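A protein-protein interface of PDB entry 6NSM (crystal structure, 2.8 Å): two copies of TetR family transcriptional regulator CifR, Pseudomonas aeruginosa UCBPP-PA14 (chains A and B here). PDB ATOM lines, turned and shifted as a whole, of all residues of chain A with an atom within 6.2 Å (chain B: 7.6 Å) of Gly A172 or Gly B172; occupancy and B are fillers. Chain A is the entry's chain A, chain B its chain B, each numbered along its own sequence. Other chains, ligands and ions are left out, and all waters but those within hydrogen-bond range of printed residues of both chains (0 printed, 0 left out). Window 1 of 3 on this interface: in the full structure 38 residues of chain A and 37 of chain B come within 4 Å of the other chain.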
ATOM      1  N   VAL A 112      34.061  29.133  20.862  1.00  0.00           N
ATOM      2  CA  VAL A 112      33.584  28.423  19.680  1.00  0.00           C
ATOM      3  C   VAL A 112      34.748  27.850  18.878  1.00  0.00           C
ATOM      4  O   VAL A 112      34.657  26.742  18.337  1.00  0.00           O
ATOM      5  CB  VAL A 112      32.689  29.350  18.834  1.00  0.00           C
ATOM      6  CG1 VAL A 112      32.512  28.800  17.424  1.00  0.00           C
ATOM      7  CG2 VAL A 112      31.339  29.549  19.511  1.00  0.00           C
ATOM      8  N   ALA A 167      21.684  32.515  19.672  1.00  0.00           N
ATOM      9  CA  ALA A 167      22.936  31.821  19.949  1.00  0.00           C
ATOM     10  C   ALA A 167      23.496  31.175  18.687  1.00  0.00           C
ATOM     11  O   ALA A 167      24.717  31.118  18.503  1.00  0.00           O
ATOM     12  CB  ALA A 167      22.726  30.778  21.044  1.00  0.00           C
ATOM     13  N   THR A 168      22.619  30.681  17.809  1.00  0.00           N
ATOM     14  CA  THR A 168      23.072  30.156  16.525  1.00  0.00           C
ATOM     15  C   THR A 168      23.741  31.250  15.704  1.00  0.00           C
ATOM     16  O   THR A 168      24.848  31.066  15.183  1.00  0.00           O
ATOM     17  CB  THR A 168      21.895  29.545  15.762  1.00  0.00           C
ATOM     18  OG1 THR A 168      21.316  28.487  16.535  1.00  0.00           O
ATOM     19  CG2 THR A 168      22.357  28.993  14.421  1.00  0.00           C
ATOM     20  N   VAL A 169      23.069  32.397  15.565  1.00  0.00           N
ATOM     21  CA  VAL A 169      23.655  33.530  14.853  1.00  0.00           C
ATOM     22  C   VAL A 169      24.963  33.949  15.508  1.00  0.00           C
ATOM     23  O   VAL A 169      25.931  34.308  14.828  1.00  0.00           O
ATOM     24  CB  VAL A 169      22.644  34.690  14.773  1.00  0.00           C
ATOM     25  CG1 VAL A 169      23.292  35.931  14.182  1.00  0.00           C
ATOM     26  CG2 VAL A 169      21.429  34.275  13.955  1.00  0.00           C
ATOM     27  N   LEU A 170      25.020  33.891  16.842  1.00  0.00           N
ATOM     28  CA  LEU A 170      26.226  34.302  17.555  1.00  0.00           C
ATOM     29  C   LEU A 170      27.387  33.358  17.269  1.00  0.00           C
ATOM     30  O   LEU A 170      28.517  33.808  17.040  1.00  0.00           O
ATOM     31  CB  LEU A 170      25.948  34.374  19.055  1.00  0.00           C
ATOM     32  CG  LEU A 170      27.152  34.634  19.960  1.00  0.00           C
ATOM     33  CD1 LEU A 170      27.642  36.064  19.804  1.00  0.00           C
ATOM     34  CD2 LEU A 170      26.800  34.335  21.408  1.00  0.00           C
ATOM     35  N   PHE A 171      27.134  32.047  17.281  1.00  0.00           N
ATOM     36  CA  PHE A 171      28.205  31.092  17.014  1.00  0.00           C
ATOM     37  C   PHE A 171      28.676  31.189  15.569  1.00  0.00           C
ATOM     38  O   PHE A 171      29.882  31.139  15.299  1.00  0.00           O
ATOM     39  CB  PHE A 171      27.751  29.668  17.343  1.00  0.00           C
ATOM     40  CG  PHE A 171      27.279  29.489  18.760  1.00  0.00           C
ATOM     41  CD1 PHE A 171      27.707  30.341  19.766  1.00  0.00           C
ATOM     42  CD2 PHE A 171      26.408  28.462  19.087  1.00  0.00           C
ATOM     43  CE1 PHE A 171      27.271  30.176  21.067  1.00  0.00           C
ATOM     44  CE2 PHE A 171      25.970  28.292  20.386  1.00  0.00           C
ATOM     45  CZ  PHE A 171      26.404  29.149  21.377  1.00  0.00           C
ATOM     46  N   GLY A 172      27.740  31.317  14.626  1.00  0.00           N
ATOM     47  CA  GLY A 172      28.110  31.491  13.234  1.00  0.00           C
ATOM     48  C   GLY A 172      28.947  32.724  12.969  1.00  0.00           C
ATOM     49  O   GLY A 172      29.700  32.752  11.990  1.00  0.00           O
ATOM     50  N   LEU A 173      28.850  33.742  13.829  1.00  0.00           N
ATOM     51  CA  LEU A 173      29.639  34.953  13.629  1.00  0.00           C
ATOM     52  C   LEU A 173      31.113  34.725  13.939  1.00  0.00           C
ATOM     53  O   LEU A 173      31.973  35.420  13.388  1.00  0.00           O
ATOM     54  CB  LEU A 173      29.082  36.105  14.463  1.00  0.00           C
ATOM     55  CG  LEU A 173      27.772  36.732  13.977  1.00  0.00           C
ATOM     56  CD1 LEU A 173      27.138  37.584  15.068  1.00  0.00           C
ATOM     57  CD2 LEU A 173      27.999  37.550  12.715  1.00  0.00           C
ATOM     58  N   SER A 174      31.424  33.764  14.812  1.00  0.00           N
ATOM     59  CA  SER A 174      32.819  33.403  15.045  1.00  0.00           C
ATOM     60  C   SER A 174      33.441  32.795  13.795  1.00  0.00           C
ATOM     61  O   SER A 174      34.593  33.093  13.457  1.00  0.00           O
ATOM     62  CB  SER A 174      32.924  32.436  16.224  1.00  0.00           C
ATOM     63  OG  SER A 174      32.480  33.042  17.425  1.00  0.00           O
ATOM     64  N   VAL A 175      32.692  31.941  13.098  1.00  0.00           N
ATOM     65  CA  VAL A 175      33.197  31.326  11.877  1.00  0.00           C
ATOM     66  C   VAL A 175      33.354  32.367  10.773  1.00  0.00           C
ATOM     67  O   VAL A 175      34.331  32.347  10.016  1.00  0.00           O
ATOM     68  CB  VAL A 175      32.291  30.156  11.455  1.00  0.00           C
ATOM     69  CG1 VAL A 175      32.810  29.521  10.190  1.00  0.00           C
ATOM     70  CG2 VAL A 175      32.202  29.127  12.571  1.00  0.00           C
ATOM     71  N   GLN A 176      32.399  33.295  10.665  1.00  0.00           N
ATOM     72  CA  GLN A 176      32.503  34.345   9.657  1.00  0.00           C
ATOM     73  C   GLN A 176      33.619  35.326   9.993  1.00  0.00           C
ATOM     74  O   GLN A 176      34.320  35.807   9.094  1.00  0.00           O
ATOM     75  CB  GLN A 176      31.168  35.071   9.498  1.00  0.00           C
ATOM     76  CG  GLN A 176      29.991  34.160   9.202  1.00  0.00           C
ATOM     77  CD  GLN A 176      29.791  33.931   7.718  1.00  0.00           C
ATOM     78  OE1 GLN A 176      30.747  33.935   6.942  1.00  0.00           O
ATOM     79  NE2 GLN A 176      28.540  33.736   7.313  1.00  0.00           N
ATOM     80  N   ALA A 177      33.795  35.644  11.279  1.00  0.00           N
ATOM     81  CA  ALA A 177      34.915  36.489  11.680  1.00  0.00           C
ATOM     82  C   ALA A 177      36.247  35.811  11.383  1.00  0.00           C
ATOM     83  O   ALA A 177      37.192  36.459  10.920  1.00  0.00           O
ATOM     84  CB  ALA A 177      34.808  36.843  13.162  1.00  0.00           C
ATOM     85  N   PHE B 100      21.770  16.959   9.905  1.00  0.00           N
ATOM     86  CA  PHE B 100      22.553  17.303  11.084  1.00  0.00           C
ATOM     87  C   PHE B 100      22.065  16.596  12.340  1.00  0.00           C
ATOM     88  O   PHE B 100      22.720  16.701  13.379  1.00  0.00           O
ATOM     89  CB  PHE B 100      22.546  18.821  11.307  1.00  0.00           C
ATOM     90  CG  PHE B 100      23.539  19.570  10.456  1.00  0.00           C
ATOM     91  CD1 PHE B 100      24.210  18.938   9.423  1.00  0.00           C
ATOM     92  CD2 PHE B 100      23.798  20.909  10.693  1.00  0.00           C
ATOM     93  CE1 PHE B 100      25.122  19.626   8.643  1.00  0.00           C
ATOM     94  CE2 PHE B 100      24.707  21.605   9.918  1.00  0.00           C
ATOM     95  CZ  PHE B 100      25.371  20.964   8.891  1.00  0.00           C
ATOM     96  N   VAL B 112      32.663  22.948   8.414  1.00  0.00           N
ATOM     97  CA  VAL B 112      32.667  23.888   9.531  1.00  0.00           C
ATOM     98  C   VAL B 112      33.519  23.372  10.689  1.00  0.00           C
ATOM     99  O   VAL B 112      34.236  24.144  11.336  1.00  0.00           O
ATOM    100  CB  VAL B 112      31.224  24.211   9.962  1.00  0.00           C
ATOM    101  CG1 VAL B 112      31.210  24.954  11.290  1.00  0.00           C
ATOM    102  CG2 VAL B 112      30.517  25.022   8.886  1.00  0.00           C
ATOM    103  N   THR B 164      24.772  36.074   3.278  1.00  0.00           N
ATOM    104  CA  THR B 164      25.684  35.936   4.411  1.00  0.00           C
ATOM    105  C   THR B 164      24.924  35.634   5.697  1.00  0.00           C
ATOM    106  O   THR B 164      25.381  34.830   6.519  1.00  0.00           O
ATOM    107  CB  THR B 164      26.531  37.200   4.561  1.00  0.00           C
ATOM    108  OG1 THR B 164      27.252  37.441   3.346  1.00  0.00           O
ATOM    109  CG2 THR B 164      27.529  37.041   5.696  1.00  0.00           C
ATOM    110  N   TYR B 166      22.051  33.978   6.109  1.00  0.00           N
ATOM    111  CA  TYR B 166      21.627  32.584   6.147  1.00  0.00           C
ATOM    112  C   TYR B 166      22.819  31.638   6.179  1.00  0.00           C
ATOM    113  O   TYR B 166      22.708  30.522   6.698  1.00  0.00           O
ATOM    114  CB  TYR B 166      20.698  32.283   4.970  1.00  0.00           C
ATOM    115  CG  TYR B 166      19.305  32.827   5.173  1.00  0.00           C
ATOM    116  CD1 TYR B 166      18.493  32.342   6.190  1.00  0.00           C
ATOM    117  CD2 TYR B 166      18.811  33.844   4.369  1.00  0.00           C
ATOM    118  CE1 TYR B 166      17.221  32.843   6.390  1.00  0.00           C
ATOM    119  CE2 TYR B 166      17.541  34.352   4.563  1.00  0.00           C
ATOM    120  CZ  TYR B 166      16.751  33.849   5.574  1.00  0.00           C
ATOM    121  OH  TYR B 166      15.484  34.350   5.771  1.00  0.00           O
ATOM    122  N   ALA B 167      23.962  32.065   5.640  1.00  0.00           N
ATOM    123  CA  ALA B 167      25.183  31.285   5.800  1.00  0.00           C
ATOM    124  C   ALA B 167      25.651  31.299   7.249  1.00  0.00           C
ATOM    125  O   ALA B 167      26.118  30.278   7.767  1.00  0.00           O
ATOM    126  CB  ALA B 167      26.273  31.816   4.870  1.00  0.00           C
ATOM    127  N   THR B 168      25.548  32.454   7.915  1.00  0.00           N
ATOM    128  CA  THR B 168      25.842  32.513   9.344  1.00  0.00           C
ATOM    129  C   THR B 168      24.973  31.529  10.116  1.00  0.00           C
ATOM    130  O   THR B 168      25.462  30.815  10.999  1.00  0.00           O
ATOM    131  CB  THR B 168      25.639  33.938   9.861  1.00  0.00           C
ATOM    132  OG1 THR B 168      26.482  34.838   9.132  1.00  0.00           O
ATOM    133  CG2 THR B 168      25.979  34.021  11.341  1.00  0.00           C
ATOM    134  N   VAL B 169      23.679  31.478   9.793  1.00  0.00           N
ATOM    135  CA  VAL B 169      22.781  30.541  10.459  1.00  0.00           C
ATOM    136  C   VAL B 169      23.176  29.108  10.128  1.00  0.00           C
ATOM    137  O   VAL B 169      23.171  28.229  10.999  1.00  0.00           O
ATOM    138  CB  VAL B 169      21.317  30.847  10.088  1.00  0.00           C
ATOM    139  CG1 VAL B 169      20.416  29.669  10.431  1.00  0.00           C
ATOM    140  CG2 VAL B 169      20.845  32.115  10.786  1.00  0.00           C
ATOM    141  N   LEU B 170      23.526  28.853   8.864  1.00  0.00           N
ATOM    142  CA  LEU B 170      23.950  27.517   8.453  1.00  0.00           C
ATOM    143  C   LEU B 170      25.170  27.062   9.243  1.00  0.00           C
ATOM    144  O   LEU B 170      25.207  25.937   9.756  1.00  0.00           O
ATOM    145  CB  LEU B 170      24.238  27.500   6.951  1.00  0.00           C
ATOM    146  CG  LEU B 170      24.816  26.204   6.374  1.00  0.00           C
ATOM    147  CD1 LEU B 170      23.863  25.039   6.583  1.00  0.00           C
ATOM    148  CD2 LEU B 170      25.143  26.370   4.899  1.00  0.00           C
ATOM    149  N   PHE B 171      26.187  27.923   9.345  1.00  0.00           N
ATOM    150  CA  PHE B 171      27.389  27.556  10.088  1.00  0.00           C
ATOM    151  C   PHE B 171      27.087  27.388  11.571  1.00  0.00           C
ATOM    152  O   PHE B 171      27.610  26.472  12.217  1.00  0.00           O
ATOM    153  CB  PHE B 171      28.487  28.599   9.876  1.00  0.00           C
ATOM    154  CG  PHE B 171      28.828  28.843   8.432  1.00  0.00           C
ATOM    155  CD1 PHE B 171      28.656  27.847   7.482  1.00  0.00           C
ATOM    156  CD2 PHE B 171      29.327  30.070   8.025  1.00  0.00           C
ATOM    157  CE1 PHE B 171      28.970  28.072   6.154  1.00  0.00           C
ATOM    158  CE2 PHE B 171      29.644  30.301   6.698  1.00  0.00           C
ATOM    159  CZ  PHE B 171      29.466  29.301   5.763  1.00  0.00           C
ATOM    160  N   GLY B 172      26.251  28.266  12.130  1.00  0.00           N
ATOM    161  CA  GLY B 172      25.892  28.142  13.532  1.00  0.00           C
ATOM    162  C   GLY B 172      25.198  26.833  13.849  1.00  0.00           C
ATOM    163  O   GLY B 172      25.349  26.297  14.949  1.00  0.00           O
ATOM    164  N   LEU B 173      24.432  26.301  12.891  1.00  0.00           N
ATOM    165  CA  LEU B 173      23.718  25.049  13.116  1.00  0.00           C
ATOM    166  C   LEU B 173      24.675  23.873  13.265  1.00  0.00           C
ATOM    167  O   LEU B 173      24.348  22.896  13.946  1.00  0.00           O
ATOM    168  CB  LEU B 173      22.725  24.792  11.983  1.00  0.00           C
ATOM    169  CG  LEU B 173      21.447  25.634  12.002  1.00  0.00           C
ATOM    170  CD1 LEU B 173      20.683  25.482  10.696  1.00  0.00           C
ATOM    171  CD2 LEU B 173      20.575  25.254  13.188  1.00  0.00           C
ATOM    172  N   SER B 174      25.852  23.943  12.636  1.00  0.00           N
ATOM    173  CA  SER B 174      26.857  22.905  12.843  1.00  0.00           C
ATOM    174  C   SER B 174      27.339  22.895  14.288  1.00  0.00           C
ATOM    175  O   SER B 174      27.490  21.827  14.892  1.00  0.00           O
ATOM    176  CB  SER B 174      28.032  23.111  11.887  1.00  0.00           C
ATOM    177  OG  SER B 174      27.646  22.885  10.542  1.00  0.00           O
ATOM    178  N   VAL B 175      27.589  24.076  14.856  1.00  0.00           N
ATOM    179  CA  VAL B 175      28.009  24.155  16.250  1.00  0.00           C
ATOM    180  C   VAL B 175      26.897  23.665  17.169  1.00  0.00           C
ATOM    181  O   VAL B 175      27.154  22.980  18.165  1.00  0.00           O
ATOM    182  CB  VAL B 175      28.468  25.584  16.586  1.00  0.00           C
ATOM    183  CG1 VAL B 175      29.050  25.640  17.988  1.00  0.00           C
ATOM    184  CG2 VAL B 175      29.485  26.067  15.562  1.00  0.00           C
ATOM    185  N   GLN B 176      25.643  23.987  16.839  1.00  0.00           N
ATOM    186  CA  GLN B 176      24.525  23.575  17.682  1.00  0.00           C
ATOM    187  C   GLN B 176      24.282  22.074  17.582  1.00  0.00           C
ATOM    188  O   GLN B 176      24.001  21.418  18.592  1.00  0.00           O
ATOM    189  CB  GLN B 176      23.267  24.355  17.301  1.00  0.00           C
ATOM    190  CG  GLN B 176      23.371  25.865  17.491  1.00  0.00           C
ATOM    191  CD  GLN B 176      23.260  26.304  18.941  1.00  0.00           C
ATOM    192  OE1 GLN B 176      23.445  25.512  19.865  1.00  0.00           O
ATOM    193  NE2 GLN B 176      22.967  27.584  19.145  1.00  0.00           N
ATOM    194  N   ALA B 177      24.369  21.519  16.369  1.00  0.00           N
ATOM    195  CA  ALA B 177      24.183  20.083  16.188  1.00  0.00           C
ATOM    196  C   ALA B 177      25.249  19.295  16.937  1.00  0.00           C
ATOM    197  O   ALA B 177      24.949  18.280  17.576  1.00  0.00           O
ATOM    198  CB  ALA B 177      24.199  19.731  14.699  1.00  0.00           C
ATOM    199  N   LYS B 178      26.506  19.743  16.861  1.00  0.00           N
ATOM    200  CA  LYS B 178      27.565  19.101  17.632  1.00  0.00           C
ATOM    201  C   LYS B 178      27.263  19.168  19.120  1.00  0.00           C
ATOM    202  O   LYS B 178      27.546  18.224  19.868  1.00  0.00           O
ATOM    203  CB  LYS B 178      28.912  19.752  17.320  1.00  0.00           C
ATOM    204  CG  LYS B 178      30.078  19.200  18.118  1.00  0.00           C
ATOM    205  CD  LYS B 178      30.927  18.269  17.267  1.00  0.00           C
ATOM    206  CE  LYS B 178      31.439  17.093  18.072  1.00  0.00           C
ATOM    207  NZ  LYS B 178      32.503  16.347  17.348  1.00  0.00           N
ATOM    208  N   ASP B 179      26.680  20.280  19.566  1.00  0.00           N
ATOM    209  CA  ASP B 179      26.300  20.432  20.964  1.00  0.00           C
ATOM    210  C   ASP B 179      25.100  19.570  21.345  1.00  0.00           C
ATOM    211  O   ASP B 179      24.618  19.670  22.482  1.00  0.00           O
ATOM    212  CB  ASP B 179      26.023  21.903  21.284  1.00  0.00           C
ATOM    213  CG  ASP B 179      27.292  22.725  21.387  1.00  0.00           C
ATOM    214  OD1 ASP B 179      28.396  22.143  21.320  1.00  0.00           O
ATOM    215  OD2 ASP B 179      27.184  23.958  21.543  1.00  0.00           O
ATOM    216  N   LEU B 186      16.297  22.804  16.540  1.00  0.00           N
ATOM    217  CA  LEU B 186      17.009  23.309  15.370  1.00  0.00           C
ATOM    218  C   LEU B 186      16.043  23.712  14.261  1.00  0.00           C
ATOM    219  O   LEU B 186      16.281  24.697  13.551  1.00  0.00           O
ATOM    220  CB  LEU B 186      18.019  22.276  14.871  1.00  0.00           C
ATOM    221  CG  LEU B 186      19.180  21.962  15.815  1.00  0.00           C
ATOM    222  CD1 LEU B 186      20.184  21.044  15.141  1.00  0.00           C
ATOM    223  CD2 LEU B 186      19.851  23.251  16.259  1.00  0.00           C
ATOM    224  N   VAL B 189      14.824  27.108  14.957  1.00  0.00           N
ATOM    225  CA  VAL B 189      15.809  28.105  14.544  1.00  0.00           C
ATOM    226  C   VAL B 189      15.635  28.440  13.069  1.00  0.00           C
ATOM    227  O   VAL B 189      15.633  29.613  12.675  1.00  0.00           O
ATOM    228  CB  VAL B 189      17.234  27.616  14.858  1.00  0.00           C
ATOM    229  CG1 VAL B 189      18.266  28.513  14.190  1.00  0.00           C
ATOM    230  CG2 VAL B 189      17.457  27.562  16.360  1.00  0.00           C
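The side-chain amide nitrogen (NE2) of Gln A176 lies within hydrogen-bond range of the backbone carbonyl oxygen (O) of Thr B164. The side-chain hydroxyl (OG1) of Thr B168 sits at hydrogen-bond distance from the side-chain amide nitrogen (NE2) of Gln A176 (3.0 Å). The side-chain hydroxyl (OG1) of Thr A168 is in hydrogen-bond range of the side-chain amide nitrogen (NE2) of Gln B176 (3.2 Å).
O of Thr B164 sits at hydrogen-bond distance from OG1 of Thr B168.
Gly A172 touches just these residues of chain B: Thr B168 (3.5 Å) and Gly B172 (3.8 Å). Of chain A, only Thr A168 (3.5 Å) and Gly A172 (3.8 Å) come within 4 Å of Gly B172. Of the printed residues of chain A, Thr B168 touches Val A169 (3.5 Å), Gly A172 (3.5 Å), Leu A173 (3.8 Å) and Gln A176 (3.0 Å). Printed residues of chain A within 4 Å of Val B189: Thr A168. Printed residues of chain B within 4 Å of Val A169: Thr B168 (3.5 Å) and Val B169 (3.9 Å). Val B112 touches none of the printed residues of chain A. The nearest residue of chain B that does not touch Gly A172 is Phe B171 (4.4 Å). The nearest residue of chain A that does not touch Gly B172 is Phe A171 (4.5 Å).
Hydrophobic or aromatic side chains of chain B within 4 Å of the printed part of chain A: Ala B167, Val B169, Phe B171 and Val B189. Among the printed residues, 16 pairs touch across the chains. Among the printed residues, no Asp or Glu carboxylate lies within 4 Å of a Lys or Arg side-chain nitrogen of the other chain.
Among the printed residues, merely in contact across the chains: Phe A171 with Gln B176 (3.3 Å), Val A169 with Thr B168 (3.5 Å), Thr A168 with Gly B172 (3.5 Å), Gly A172 with Thr B168 (3.5 Å), Thr A168 with Val B169 (3.6 Å), Ala A167 with Gln B176 (3.7 Å), Gln A176 with Phe B171 (3.7 Å), Thr A168 with Leu B173 (3.7 Å), Gln A176 with Ala B167 (3.8 Å), Leu A173 with Thr B168 (3.8 Å), Gly A172 with Gly B172 (3.8 Å), Thr A168 with Val B189 (3.8 Å) and Val A169 with Val B169 (3.9 Å).
Thr A168 touches Gly B172, and with the chains exchanged Gly A172 touches Thr B168. Val A169 touches its own counterpart, Val B169. Phe A171 touches Gln B176, and with the chains exchanged Gln A176 touches Phe B171. Gly B172 touches its own counterpart, Gly A172.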
